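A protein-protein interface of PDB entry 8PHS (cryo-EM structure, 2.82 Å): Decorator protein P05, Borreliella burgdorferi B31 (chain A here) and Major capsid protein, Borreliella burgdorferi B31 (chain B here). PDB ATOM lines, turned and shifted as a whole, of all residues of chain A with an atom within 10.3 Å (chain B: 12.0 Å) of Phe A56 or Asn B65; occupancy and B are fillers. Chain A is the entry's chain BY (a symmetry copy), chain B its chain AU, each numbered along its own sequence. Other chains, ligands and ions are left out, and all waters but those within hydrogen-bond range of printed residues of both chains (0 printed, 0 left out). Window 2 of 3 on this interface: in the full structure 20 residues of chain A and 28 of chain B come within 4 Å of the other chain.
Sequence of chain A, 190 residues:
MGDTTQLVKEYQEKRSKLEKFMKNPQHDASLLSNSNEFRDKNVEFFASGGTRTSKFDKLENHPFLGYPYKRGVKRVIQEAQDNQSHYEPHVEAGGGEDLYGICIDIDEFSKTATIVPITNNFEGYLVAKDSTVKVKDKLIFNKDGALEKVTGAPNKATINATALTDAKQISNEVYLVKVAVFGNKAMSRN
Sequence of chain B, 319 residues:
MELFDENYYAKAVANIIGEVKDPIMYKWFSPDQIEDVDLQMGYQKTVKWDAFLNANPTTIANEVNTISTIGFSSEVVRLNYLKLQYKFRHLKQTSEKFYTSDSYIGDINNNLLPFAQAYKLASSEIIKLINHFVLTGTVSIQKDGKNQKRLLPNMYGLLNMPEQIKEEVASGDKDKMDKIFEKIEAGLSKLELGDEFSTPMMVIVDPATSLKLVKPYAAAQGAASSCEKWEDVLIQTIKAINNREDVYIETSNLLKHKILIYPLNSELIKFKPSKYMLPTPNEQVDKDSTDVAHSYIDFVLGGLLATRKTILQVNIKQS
Phe A56 touches just one residue of chain B: Asn B65. Asn B65 touches just these residues of chain A: Thr A53 (3.8 Å), Ser A54 (3.0 Å), Lys A55 (3.96 Å) and Phe A56 (3.5 Å). Of chain A, only Arg A52 and Thr A53 come within 4 Å of Ile B67. Printed residues of chain B within 4 Å of Thr A53: Asn B65 (3.8 Å), Ile B67 (3.1 Å) and Thr B69 (3.99 Å). Printed residues of chain B within 4 Å of Thr A51: Ser B68 (3.4 Å) and Thr B69 (2.9 Å). Ala B61 touches none of the printed residues of chain A. The nearest printed residue of chain A that does not touch Ser B68 is Thr A53 (5.1 Å).
The side-chain amide oxygen (OD1) of Asn B65 sits at hydrogen-bond distance from the side-chain hydroxyl (OG) of Ser A54 (3.0 Å). The backbone carbonyl oxygen (O) of Ile B67 sits at hydrogen-bond distance from the backbone NH (N) of Thr A53. The backbone NH of Thr B69 sits at hydrogen-bond distance from the backbone carbonyl oxygen of Thr A51 (2.9 Å).
OG of Ser B68 sits at hydrogen-bond distance from O of Asn B56, at 2.8 Å. The side-chain hydroxyl of Thr B58 is in hydrogen-bond range of the backbone NH of Ser B68 (3.2 Å). N of Phe A56 sits close to OG of Ser A54 (3.3 Å). N of Ser A54 is in hydrogen-bond range of OD2 of Asp A57 (3.2 Å).
Hydrophobic or aromatic side chains of chain A within 4 Å of the printed part of chain B: Phe A56. Along chain A the printed residues that touch a printed residue of chain B span positions 51 to 56. Along chain B the printed residues that touch a printed residue of chain A span positions 65 to 69. Among the printed residues, 12 pairs touch across the chains.
Among the printed residues, pairs that only touch across the chains: Arg A52 with Ile B67 (3.4 Å), Arg A52 with Ser B68 (3.4 Å), Thr A51 with Ser B68 (3.4 Å), Phe A56 with Asn B65 (3.5 Å), Ser A54 with Thr B66 (3.6 Å), Thr A53 with Asn B65 (3.8 Å), Arg A52 with Thr B66 (3.9 Å), Lys A55 with Asn B65 (3.96 Å) and Thr A53 with Thr B69 (3.99 Å).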
ATOM      1  N   THR A  51     -10.852  -2.914  -8.180  1.00  0.00           N
ATOM      2  CA  THR A  51     -10.114  -2.698  -6.941  1.00  0.00           C
ATOM      3  C   THR A  51     -11.046  -2.250  -5.823  1.00  0.00           C
ATOM      4  O   THR A  51     -10.920  -2.703  -4.679  1.00  0.00           O
ATOM      5  CB  THR A  51      -9.004  -1.671  -7.162  1.00  0.00           C
ATOM      6  OG1 THR A  51      -9.577  -0.432  -7.595  1.00  0.00           O
ATOM      7  CG2 THR A  51      -8.031  -2.167  -8.219  1.00  0.00           C
ATOM      8  N   ARG A  52     -11.986  -1.361  -6.136  1.00  0.00           N
ATOM      9  CA  ARG A  52     -13.033  -0.951  -5.211  1.00  0.00           C
ATOM     10  C   ARG A  52     -14.375  -1.147  -5.895  1.00  0.00           C
ATOM     11  O   ARG A  52     -14.588  -0.644  -7.002  1.00  0.00           O
ATOM     12  CB  ARG A  52     -12.862   0.507  -4.783  1.00  0.00           C
ATOM     13  CG  ARG A  52     -11.489   0.837  -4.232  1.00  0.00           C
ATOM     14  CD  ARG A  52     -11.227   2.323  -4.336  1.00  0.00           C
ATOM     15  NE  ARG A  52     -12.387   3.098  -3.913  1.00  0.00           N
ATOM     16  CZ  ARG A  52     -12.529   4.399  -4.114  1.00  0.00           C
ATOM     17  NH1 ARG A  52     -11.609   5.103  -4.753  1.00  0.00           N
ATOM     18  NH2 ARG A  52     -13.625   5.010  -3.672  1.00  0.00           N
ATOM     19  N   THR A  53     -15.273  -1.874  -5.238  1.00  0.00           N
ATOM     20  CA  THR A  53     -16.554  -2.243  -5.825  1.00  0.00           C
ATOM     21  C   THR A  53     -17.679  -1.859  -4.877  1.00  0.00           C
ATOM     22  O   THR A  53     -17.595  -2.112  -3.672  1.00  0.00           O
ATOM     23  CB  THR A  53     -16.606  -3.745  -6.126  1.00  0.00           C
ATOM     24  OG1 THR A  53     -15.573  -4.081  -7.060  1.00  0.00           O
ATOM     25  CG2 THR A  53     -17.954  -4.127  -6.715  1.00  0.00           C
ATOM     26  N   SER A  54     -18.724  -1.249  -5.424  1.00  0.00           N
ATOM     27  CA  SER A  54     -19.916  -0.906  -4.666  1.00  0.00           C
ATOM     28  C   SER A  54     -20.982  -1.978  -4.857  1.00  0.00           C
ATOM     29  O   SER A  54     -21.067  -2.614  -5.910  1.00  0.00           O
ATOM     30  CB  SER A  54     -20.466   0.455  -5.096  1.00  0.00           C
ATOM     31  OG  SER A  54     -21.704   0.725  -4.466  1.00  0.00           O
ATOM     32  N   LYS A  55     -21.792  -2.178  -3.817  1.00  0.00           N
ATOM     33  CA  LYS A  55     -22.876  -3.151  -3.902  1.00  0.00           C
ATOM     34  C   LYS A  55     -23.898  -2.753  -4.959  1.00  0.00           C
ATOM     35  O   LYS A  55     -24.539  -3.622  -5.563  1.00  0.00           O
ATOM     36  CB  LYS A  55     -23.547  -3.302  -2.535  1.00  0.00           C
ATOM     37  CG  LYS A  55     -24.849  -4.083  -2.551  1.00  0.00           C
ATOM     38  CD  LYS A  55     -25.587  -3.972  -1.229  1.00  0.00           C
ATOM     39  CE  LYS A  55     -26.902  -4.732  -1.274  1.00  0.00           C
ATOM     40  NZ  LYS A  55     -27.644  -4.647   0.014  1.00  0.00           N
ATOM     41  N   PHE A  56     -24.043  -1.454  -5.220  1.00  0.00           N
ATOM     42  CA  PHE A  56     -25.042  -0.942  -6.146  1.00  0.00           C
ATOM     43  C   PHE A  56     -24.506  -0.782  -7.562  1.00  0.00           C
ATOM     44  O   PHE A  56     -24.979   0.084  -8.309  1.00  0.00           O
ATOM     45  CB  PHE A  56     -25.596   0.386  -5.630  1.00  0.00           C
ATOM     46  CG  PHE A  56     -26.093   0.318  -4.217  1.00  0.00           C
ATOM     47  CD1 PHE A  56     -27.121  -0.543  -3.872  1.00  0.00           C
ATOM     48  CD2 PHE A  56     -25.526   1.103  -3.231  1.00  0.00           C
ATOM     49  CE1 PHE A  56     -27.577  -0.610  -2.572  1.00  0.00           C
ATOM     50  CE2 PHE A  56     -25.978   1.038  -1.930  1.00  0.00           C
ATOM     51  CZ  PHE A  56     -27.005   0.180  -1.599  1.00  0.00           C
ATOM     52  N   ASP A  57     -23.528  -1.595  -7.953  1.00  0.00           N
ATOM     53  CA  ASP A  57     -23.000  -1.577  -9.309  1.00  0.00           C
ATOM     54  C   ASP A  57     -23.845  -2.479 -10.197  1.00  0.00           C
ATOM     55  O   ASP A  57     -24.042  -3.658  -9.886  1.00  0.00           O
ATOM     56  CB  ASP A  57     -21.543  -2.039  -9.329  1.00  0.00           C
ATOM     57  CG  ASP A  57     -20.606  -1.043  -8.677  1.00  0.00           C
ATOM     58  OD1 ASP A  57     -21.064   0.062  -8.323  1.00  0.00           O
ATOM     59  OD2 ASP A  57     -19.411  -1.368  -8.517  1.00  0.00           O
ATOM     60  N   LYS A  58     -24.345  -1.923 -11.297  1.00  0.00           N
ATOM     61  CA  LYS A  58     -25.134  -2.694 -12.249  1.00  0.00           C
ATOM     62  C   LYS A  58     -24.207  -3.566 -13.086  1.00  0.00           C
ATOM     63  O   LYS A  58     -23.282  -3.059 -13.730  1.00  0.00           O
ATOM     64  CB  LYS A  58     -25.955  -1.763 -13.136  1.00  0.00           C
ATOM     65  CG  LYS A  58     -26.925  -2.483 -14.051  1.00  0.00           C
ATOM     66  CD  LYS A  58     -27.830  -1.503 -14.773  1.00  0.00           C
ATOM     67  CE  LYS A  58     -28.889  -2.229 -15.585  1.00  0.00           C
ATOM     68  NZ  LYS A  58     -29.870  -1.286 -16.187  1.00  0.00           N
ATOM     69  N   LEU A  59     -24.452  -4.873 -13.078  1.00  0.00           N
ATOM     70  CA  LEU A  59     -23.643  -5.840 -13.809  1.00  0.00           C
ATOM     71  C   LEU A  59     -24.546  -6.621 -14.750  1.00  0.00           C
ATOM     72  O   LEU A  59     -25.520  -7.239 -14.307  1.00  0.00           O
ATOM     73  CB  LEU A  59     -22.924  -6.790 -12.849  1.00  0.00           C
ATOM     74  CG  LEU A  59     -22.070  -6.149 -11.757  1.00  0.00           C
ATOM     75  CD1 LEU A  59     -21.447  -7.215 -10.872  1.00  0.00           C
ATOM     76  CD2 LEU A  59     -20.998  -5.266 -12.369  1.00  0.00           C
ATOM     77  N   GLU A  60     -24.226  -6.597 -16.040  1.00  0.00           N
ATOM     78  CA  GLU A  60     -24.971  -7.344 -17.041  1.00  0.00           C
ATOM     79  C   GLU A  60     -24.124  -8.507 -17.540  1.00  0.00           C
ATOM     80  O   GLU A  60     -22.911  -8.547 -17.333  1.00  0.00           O
ATOM     81  CB  GLU A  60     -25.376  -6.434 -18.202  1.00  0.00           C
ATOM     82  CG  GLU A  60     -26.035  -5.145 -17.746  1.00  0.00           C
ATOM     83  CD  GLU A  60     -26.428  -4.245 -18.895  1.00  0.00           C
ATOM     84  OE1 GLU A  60     -26.152  -4.604 -20.057  1.00  0.00           O
ATOM     85  OE2 GLU A  60     -27.014  -3.172 -18.637  1.00  0.00           O
ATOM     86  N   VAL A 116     -19.890  -4.000 -17.231  1.00  0.00           N
ATOM     87  CA  VAL A 116     -20.307  -2.803 -16.508  1.00  0.00           C
ATOM     88  C   VAL A 116     -20.707  -1.760 -17.545  1.00  0.00           C
ATOM     89  O   VAL A 116     -19.860  -1.363 -18.360  1.00  0.00           O
ATOM     90  CB  VAL A 116     -19.188  -2.273 -15.599  1.00  0.00           C
ATOM     91  CG1 VAL A 116     -19.616  -0.977 -14.933  1.00  0.00           C
ATOM     92  CG2 VAL A 116     -18.809  -3.317 -14.565  1.00  0.00           C
ATOM     93  N   PRO A 117     -21.961  -1.310 -17.570  1.00  0.00           N
ATOM     94  CA  PRO A 117     -22.369  -0.331 -18.582  1.00  0.00           C
ATOM     95  C   PRO A 117     -21.605   0.974 -18.432  1.00  0.00           C
ATOM     96  O   PRO A 117     -21.176   1.346 -17.339  1.00  0.00           O
ATOM     97  CB  PRO A 117     -23.866  -0.139 -18.310  1.00  0.00           C
ATOM     98  CG  PRO A 117     -24.276  -1.344 -17.532  1.00  0.00           C
ATOM     99  CD  PRO A 117     -23.083  -1.720 -16.713  1.00  0.00           C
ATOM    100  N   THR A 119     -22.615   3.840 -18.400  1.00  0.00           N
ATOM    101  CA  THR A 119     -23.280   4.772 -17.499  1.00  0.00           C
ATOM    102  C   THR A 119     -22.882   4.569 -16.045  1.00  0.00           C
ATOM    103  O   THR A 119     -23.243   5.397 -15.202  1.00  0.00           O
ATOM    104  CB  THR A 119     -24.797   4.645 -17.637  1.00  0.00           C
ATOM    105  OG1 THR A 119     -25.196   3.301 -17.341  1.00  0.00           O
ATOM    106  CG2 THR A 119     -25.232   4.999 -19.046  1.00  0.00           C
ATOM    107  N   ASN A 120     -22.162   3.497 -15.729  1.00  0.00           N
ATOM    108  CA  ASN A 120     -21.703   3.213 -14.377  1.00  0.00           C
ATOM    109  C   ASN A 120     -20.187   3.343 -14.327  1.00  0.00           C
ATOM    110  O   ASN A 120     -19.487   2.815 -15.196  1.00  0.00           O
ATOM    111  CB  ASN A 120     -22.133   1.811 -13.940  1.00  0.00           C
ATOM    112  CG  ASN A 120     -21.957   1.582 -12.454  1.00  0.00           C
ATOM    113  OD1 ASN A 120     -21.629   2.503 -11.708  1.00  0.00           O
ATOM    114  ND2 ASN A 120     -22.177   0.349 -12.017  1.00  0.00           N
ATOM    115  N   ASN A 121     -19.685   4.041 -13.312  1.00  0.00           N
ATOM    116  CA  ASN A 121     -18.254   4.271 -13.191  1.00  0.00           C
ATOM    117  C   ASN A 121     -17.541   3.015 -12.707  1.00  0.00           C
ATOM    118  O   ASN A 121     -18.101   2.195 -11.972  1.00  0.00           O
ATOM    119  CB  ASN A 121     -17.971   5.434 -12.239  1.00  0.00           C
ATOM    120  CG  ASN A 121     -18.256   5.086 -10.795  1.00  0.00           C
ATOM    121  OD1 ASN A 121     -19.376   4.723 -10.443  1.00  0.00           O
ATOM    122  ND2 ASN A 121     -17.239   5.197  -9.949  1.00  0.00           N
ATOM    123  N   ASN B  56      -5.539   0.026  -0.893  1.00  0.00           N
ATOM    124  CA  ASN B  56      -5.506   0.408   0.507  1.00  0.00           C
ATOM    125  C   ASN B  56      -6.895   0.247   1.121  1.00  0.00           C
ATOM    126  O   ASN B  56      -7.907   0.378   0.427  1.00  0.00           O
ATOM    127  CB  ASN B  56      -5.035   1.851   0.661  1.00  0.00           C
ATOM    128  CG  ASN B  56      -3.629   2.064   0.143  1.00  0.00           C
ATOM    129  OD1 ASN B  56      -2.707   1.336   0.504  1.00  0.00           O
ATOM    130  ND2 ASN B  56      -3.456   3.071  -0.704  1.00  0.00           N
ATOM    131  N   PRO B  57      -6.973  -0.045   2.419  1.00  0.00           N
ATOM    132  CA  PRO B  57      -8.281  -0.199   3.066  1.00  0.00           C
ATOM    133  C   PRO B  57      -9.095   1.083   2.982  1.00  0.00           C
ATOM    134  O   PRO B  57      -8.601   2.157   2.635  1.00  0.00           O
ATOM    135  CB  PRO B  57      -7.929  -0.550   4.516  1.00  0.00           C
ATOM    136  CG  PRO B  57      -6.505  -0.130   4.685  1.00  0.00           C
ATOM    137  CD  PRO B  57      -5.865  -0.311   3.350  1.00  0.00           C
ATOM    138  N   THR B  58     -10.378   0.956   3.300  1.00  0.00           N
ATOM    139  CA  THR B  58     -11.326   2.058   3.210  1.00  0.00           C
ATOM    140  C   THR B  58     -11.635   2.577   4.605  1.00  0.00           C
ATOM    141  O   THR B  58     -11.936   1.794   5.511  1.00  0.00           O
ATOM    142  CB  THR B  58     -12.611   1.616   2.507  1.00  0.00           C
ATOM    143  OG1 THR B  58     -12.334   1.354   1.126  1.00  0.00           O
ATOM    144  CG2 THR B  58     -13.674   2.696   2.603  1.00  0.00           C
ATOM    145  N   THR B  59     -11.552   3.895   4.775  1.00  0.00           N
ATOM    146  CA  THR B  59     -11.896   4.526   6.043  1.00  0.00           C
ATOM    147  C   THR B  59     -13.411   4.598   6.175  1.00  0.00           C
ATOM    148  O   THR B  59     -14.082   5.241   5.360  1.00  0.00           O
ATOM    149  CB  THR B  59     -11.284   5.922   6.133  1.00  0.00           C
ATOM    150  OG1 THR B  59      -9.867   5.839   5.940  1.00  0.00           O
ATOM    151  CG2 THR B  59     -11.568   6.540   7.491  1.00  0.00           C
ATOM    152  N   ILE B  60     -13.951   3.947   7.202  1.00  0.00           N
ATOM    153  CA  ILE B  60     -15.391   3.907   7.432  1.00  0.00           C
ATOM    154  C   ILE B  60     -15.765   5.175   8.190  1.00  0.00           C
ATOM    155  O   ILE B  60     -15.496   5.306   9.385  1.00  0.00           O
ATOM    156  CB  ILE B  60     -15.810   2.647   8.189  1.00  0.00           C
ATOM    157  CG1 ILE B  60     -15.526   1.408   7.344  1.00  0.00           C
ATOM    158  CG2 ILE B  60     -17.284   2.711   8.549  1.00  0.00           C
ATOM    159  CD1 ILE B  60     -16.187   1.439   5.987  1.00  0.00           C
ATOM    160  N   ALA B  61     -16.389   6.116   7.487  1.00  0.00           N
ATOM    161  CA  ALA B  61     -16.824   7.369   8.088  1.00  0.00           C
ATOM    162  C   ALA B  61     -18.022   7.888   7.314  1.00  0.00           C
ATOM    163  O   ALA B  61     -17.980   7.959   6.082  1.00  0.00           O
ATOM    164  CB  ALA B  61     -15.695   8.404   8.087  1.00  0.00           C
ATOM    165  N   ASN B  62     -19.078   8.247   8.038  1.00  0.00           N
ATOM    166  CA  ASN B  62     -20.328   8.764   7.454  1.00  0.00           C
ATOM    167  C   ASN B  62     -20.889   7.681   6.531  1.00  0.00           C
ATOM    168  O   ASN B  62     -20.918   6.503   6.920  1.00  0.00           O
ATOM    169  CB  ASN B  62     -20.071  10.111   6.796  1.00  0.00           C
ATOM    170  CG  ASN B  62     -19.927  11.232   7.804  1.00  0.00           C
ATOM    171  OD1 ASN B  62     -20.137  11.037   9.001  1.00  0.00           O
ATOM    172  ND2 ASN B  62     -19.569  12.417   7.325  1.00  0.00           N
ATOM    173  N   GLU B  63     -21.335   8.021   5.326  1.00  0.00           N
ATOM    174  CA  GLU B  63     -21.945   7.073   4.404  1.00  0.00           C
ATOM    175  C   GLU B  63     -20.971   6.749   3.281  1.00  0.00           C
ATOM    176  O   GLU B  63     -20.377   7.657   2.691  1.00  0.00           O
ATOM    177  CB  GLU B  63     -23.242   7.636   3.821  1.00  0.00           C
ATOM    178  CG  GLU B  63     -24.291   7.996   4.853  1.00  0.00           C
ATOM    179  CD  GLU B  63     -25.547   8.560   4.223  1.00  0.00           C
ATOM    180  OE1 GLU B  63     -26.145   7.872   3.368  1.00  0.00           O
ATOM    181  OE2 GLU B  63     -25.937   9.692   4.580  1.00  0.00           O
ATOM    182  N   VAL B  64     -20.810   5.461   2.994  1.00  0.00           N
ATOM    183  CA  VAL B  64     -19.981   5.009   1.881  1.00  0.00           C
ATOM    184  C   VAL B  64     -20.342   3.559   1.585  1.00  0.00           C
ATOM    185  O   VAL B  64     -20.590   2.768   2.499  1.00  0.00           O
ATOM    186  CB  VAL B  64     -18.474   5.182   2.192  1.00  0.00           C
ATOM    187  CG1 VAL B  64     -18.075   4.377   3.419  1.00  0.00           C
ATOM    188  CG2 VAL B  64     -17.629   4.794   0.991  1.00  0.00           C
ATOM    189  N   ASN B  65     -20.392   3.220   0.295  1.00  0.00           N
ATOM    190  CA  ASN B  65     -20.612   1.844  -0.124  1.00  0.00           C
ATOM    191  C   ASN B  65     -19.594   1.331  -1.131  1.00  0.00           C
ATOM    192  O   ASN B  65     -19.624   0.138  -1.449  1.00  0.00           O
ATOM    193  CB  ASN B  65     -22.024   1.669  -0.709  1.00  0.00           C
ATOM    194  CG  ASN B  65     -22.404   2.780  -1.662  1.00  0.00           C
ATOM    195  OD1 ASN B  65     -21.700   3.050  -2.634  1.00  0.00           O
ATOM    196  ND2 ASN B  65     -23.531   3.425  -1.393  1.00  0.00           N
ATOM    197  N   THR B  66     -18.698   2.178  -1.637  1.00  0.00           N
ATOM    198  CA  THR B  66     -17.612   1.740  -2.506  1.00  0.00           C
ATOM    199  C   THR B  66     -16.411   1.411  -1.629  1.00  0.00           C
ATOM    200  O   THR B  66     -15.831   2.301  -0.999  1.00  0.00           O
ATOM    201  CB  THR B  66     -17.268   2.814  -3.533  1.00  0.00           C
ATOM    202  OG1 THR B  66     -18.471   3.291  -4.145  1.00  0.00           O
ATOM    203  CG2 THR B  66     -16.352   2.248  -4.605  1.00  0.00           C
ATOM    204  N   ILE B  67     -16.037   0.136  -1.588  1.00  0.00           N
ATOM    205  CA  ILE B  67     -15.080  -0.374  -0.616  1.00  0.00           C
ATOM    206  C   ILE B  67     -14.023  -1.195  -1.341  1.00  0.00           C
ATOM    207  O   ILE B  67     -14.338  -1.945  -2.271  1.00  0.00           O
ATOM    208  CB  ILE B  67     -15.794  -1.215   0.462  1.00  0.00           C
ATOM    209  CG1 ILE B  67     -16.804  -0.343   1.208  1.00  0.00           C
ATOM    210  CG2 ILE B  67     -14.797  -1.826   1.431  1.00  0.00           C
ATOM    211  CD1 ILE B  67     -17.443  -1.017   2.376  1.00  0.00           C
ATOM    212  N   SER B  68     -12.769  -1.043  -0.921  1.00  0.00           N
ATOM    213  CA  SER B  68     -11.679  -1.812  -1.505  1.00  0.00           C
ATOM    214  C   SER B  68     -11.880  -3.301  -1.248  1.00  0.00           C
ATOM    215  O   SER B  68     -12.412  -3.711  -0.214  1.00  0.00           O
ATOM    216  CB  SER B  68     -10.338  -1.356  -0.933  1.00  0.00           C
ATOM    217  OG  SER B  68     -10.069  -0.011  -1.283  1.00  0.00           O
ATOM    218  N   THR B  69     -11.440  -4.113  -2.203  1.00  0.00           N
ATOM    219  CA  THR B  69     -11.713  -5.541  -2.201  1.00  0.00           C
ATOM    220  C   THR B  69     -10.441  -6.347  -1.977  1.00  0.00           C
ATOM    221  O   THR B  69      -9.327  -5.891  -2.248  1.00  0.00           O
ATOM    222  CB  THR B  69     -12.367  -5.971  -3.519  1.00  0.00           C
ATOM    223  OG1 THR B  69     -11.475  -5.701  -4.608  1.00  0.00           O
ATOM    224  CG2 THR B  69     -13.666  -5.216  -3.739  1.00  0.00           C
ATOM    225  N   ILE B  70     -10.630  -7.563  -1.473  1.00  0.00           N
ATOM    226  CA  ILE B  70      -9.562  -8.542  -1.308  1.00  0.00           C
ATOM    227  C   ILE B  70      -9.803  -9.654  -2.318  1.00  0.00           C
ATOM    228  O   ILE B  70     -10.886 -10.252  -2.345  1.00  0.00           O
ATOM    229  CB  ILE B  70      -9.516  -9.101   0.123  1.00  0.00           C
ATOM    230  CG1 ILE B  70      -9.001  -8.044   1.099  1.00  0.00           C
ATOM    231  CG2 ILE B  70      -8.658 -10.353   0.181  1.00  0.00           C
ATOM    232  CD1 ILE B  70      -8.988  -8.508   2.538  1.00  0.00           C
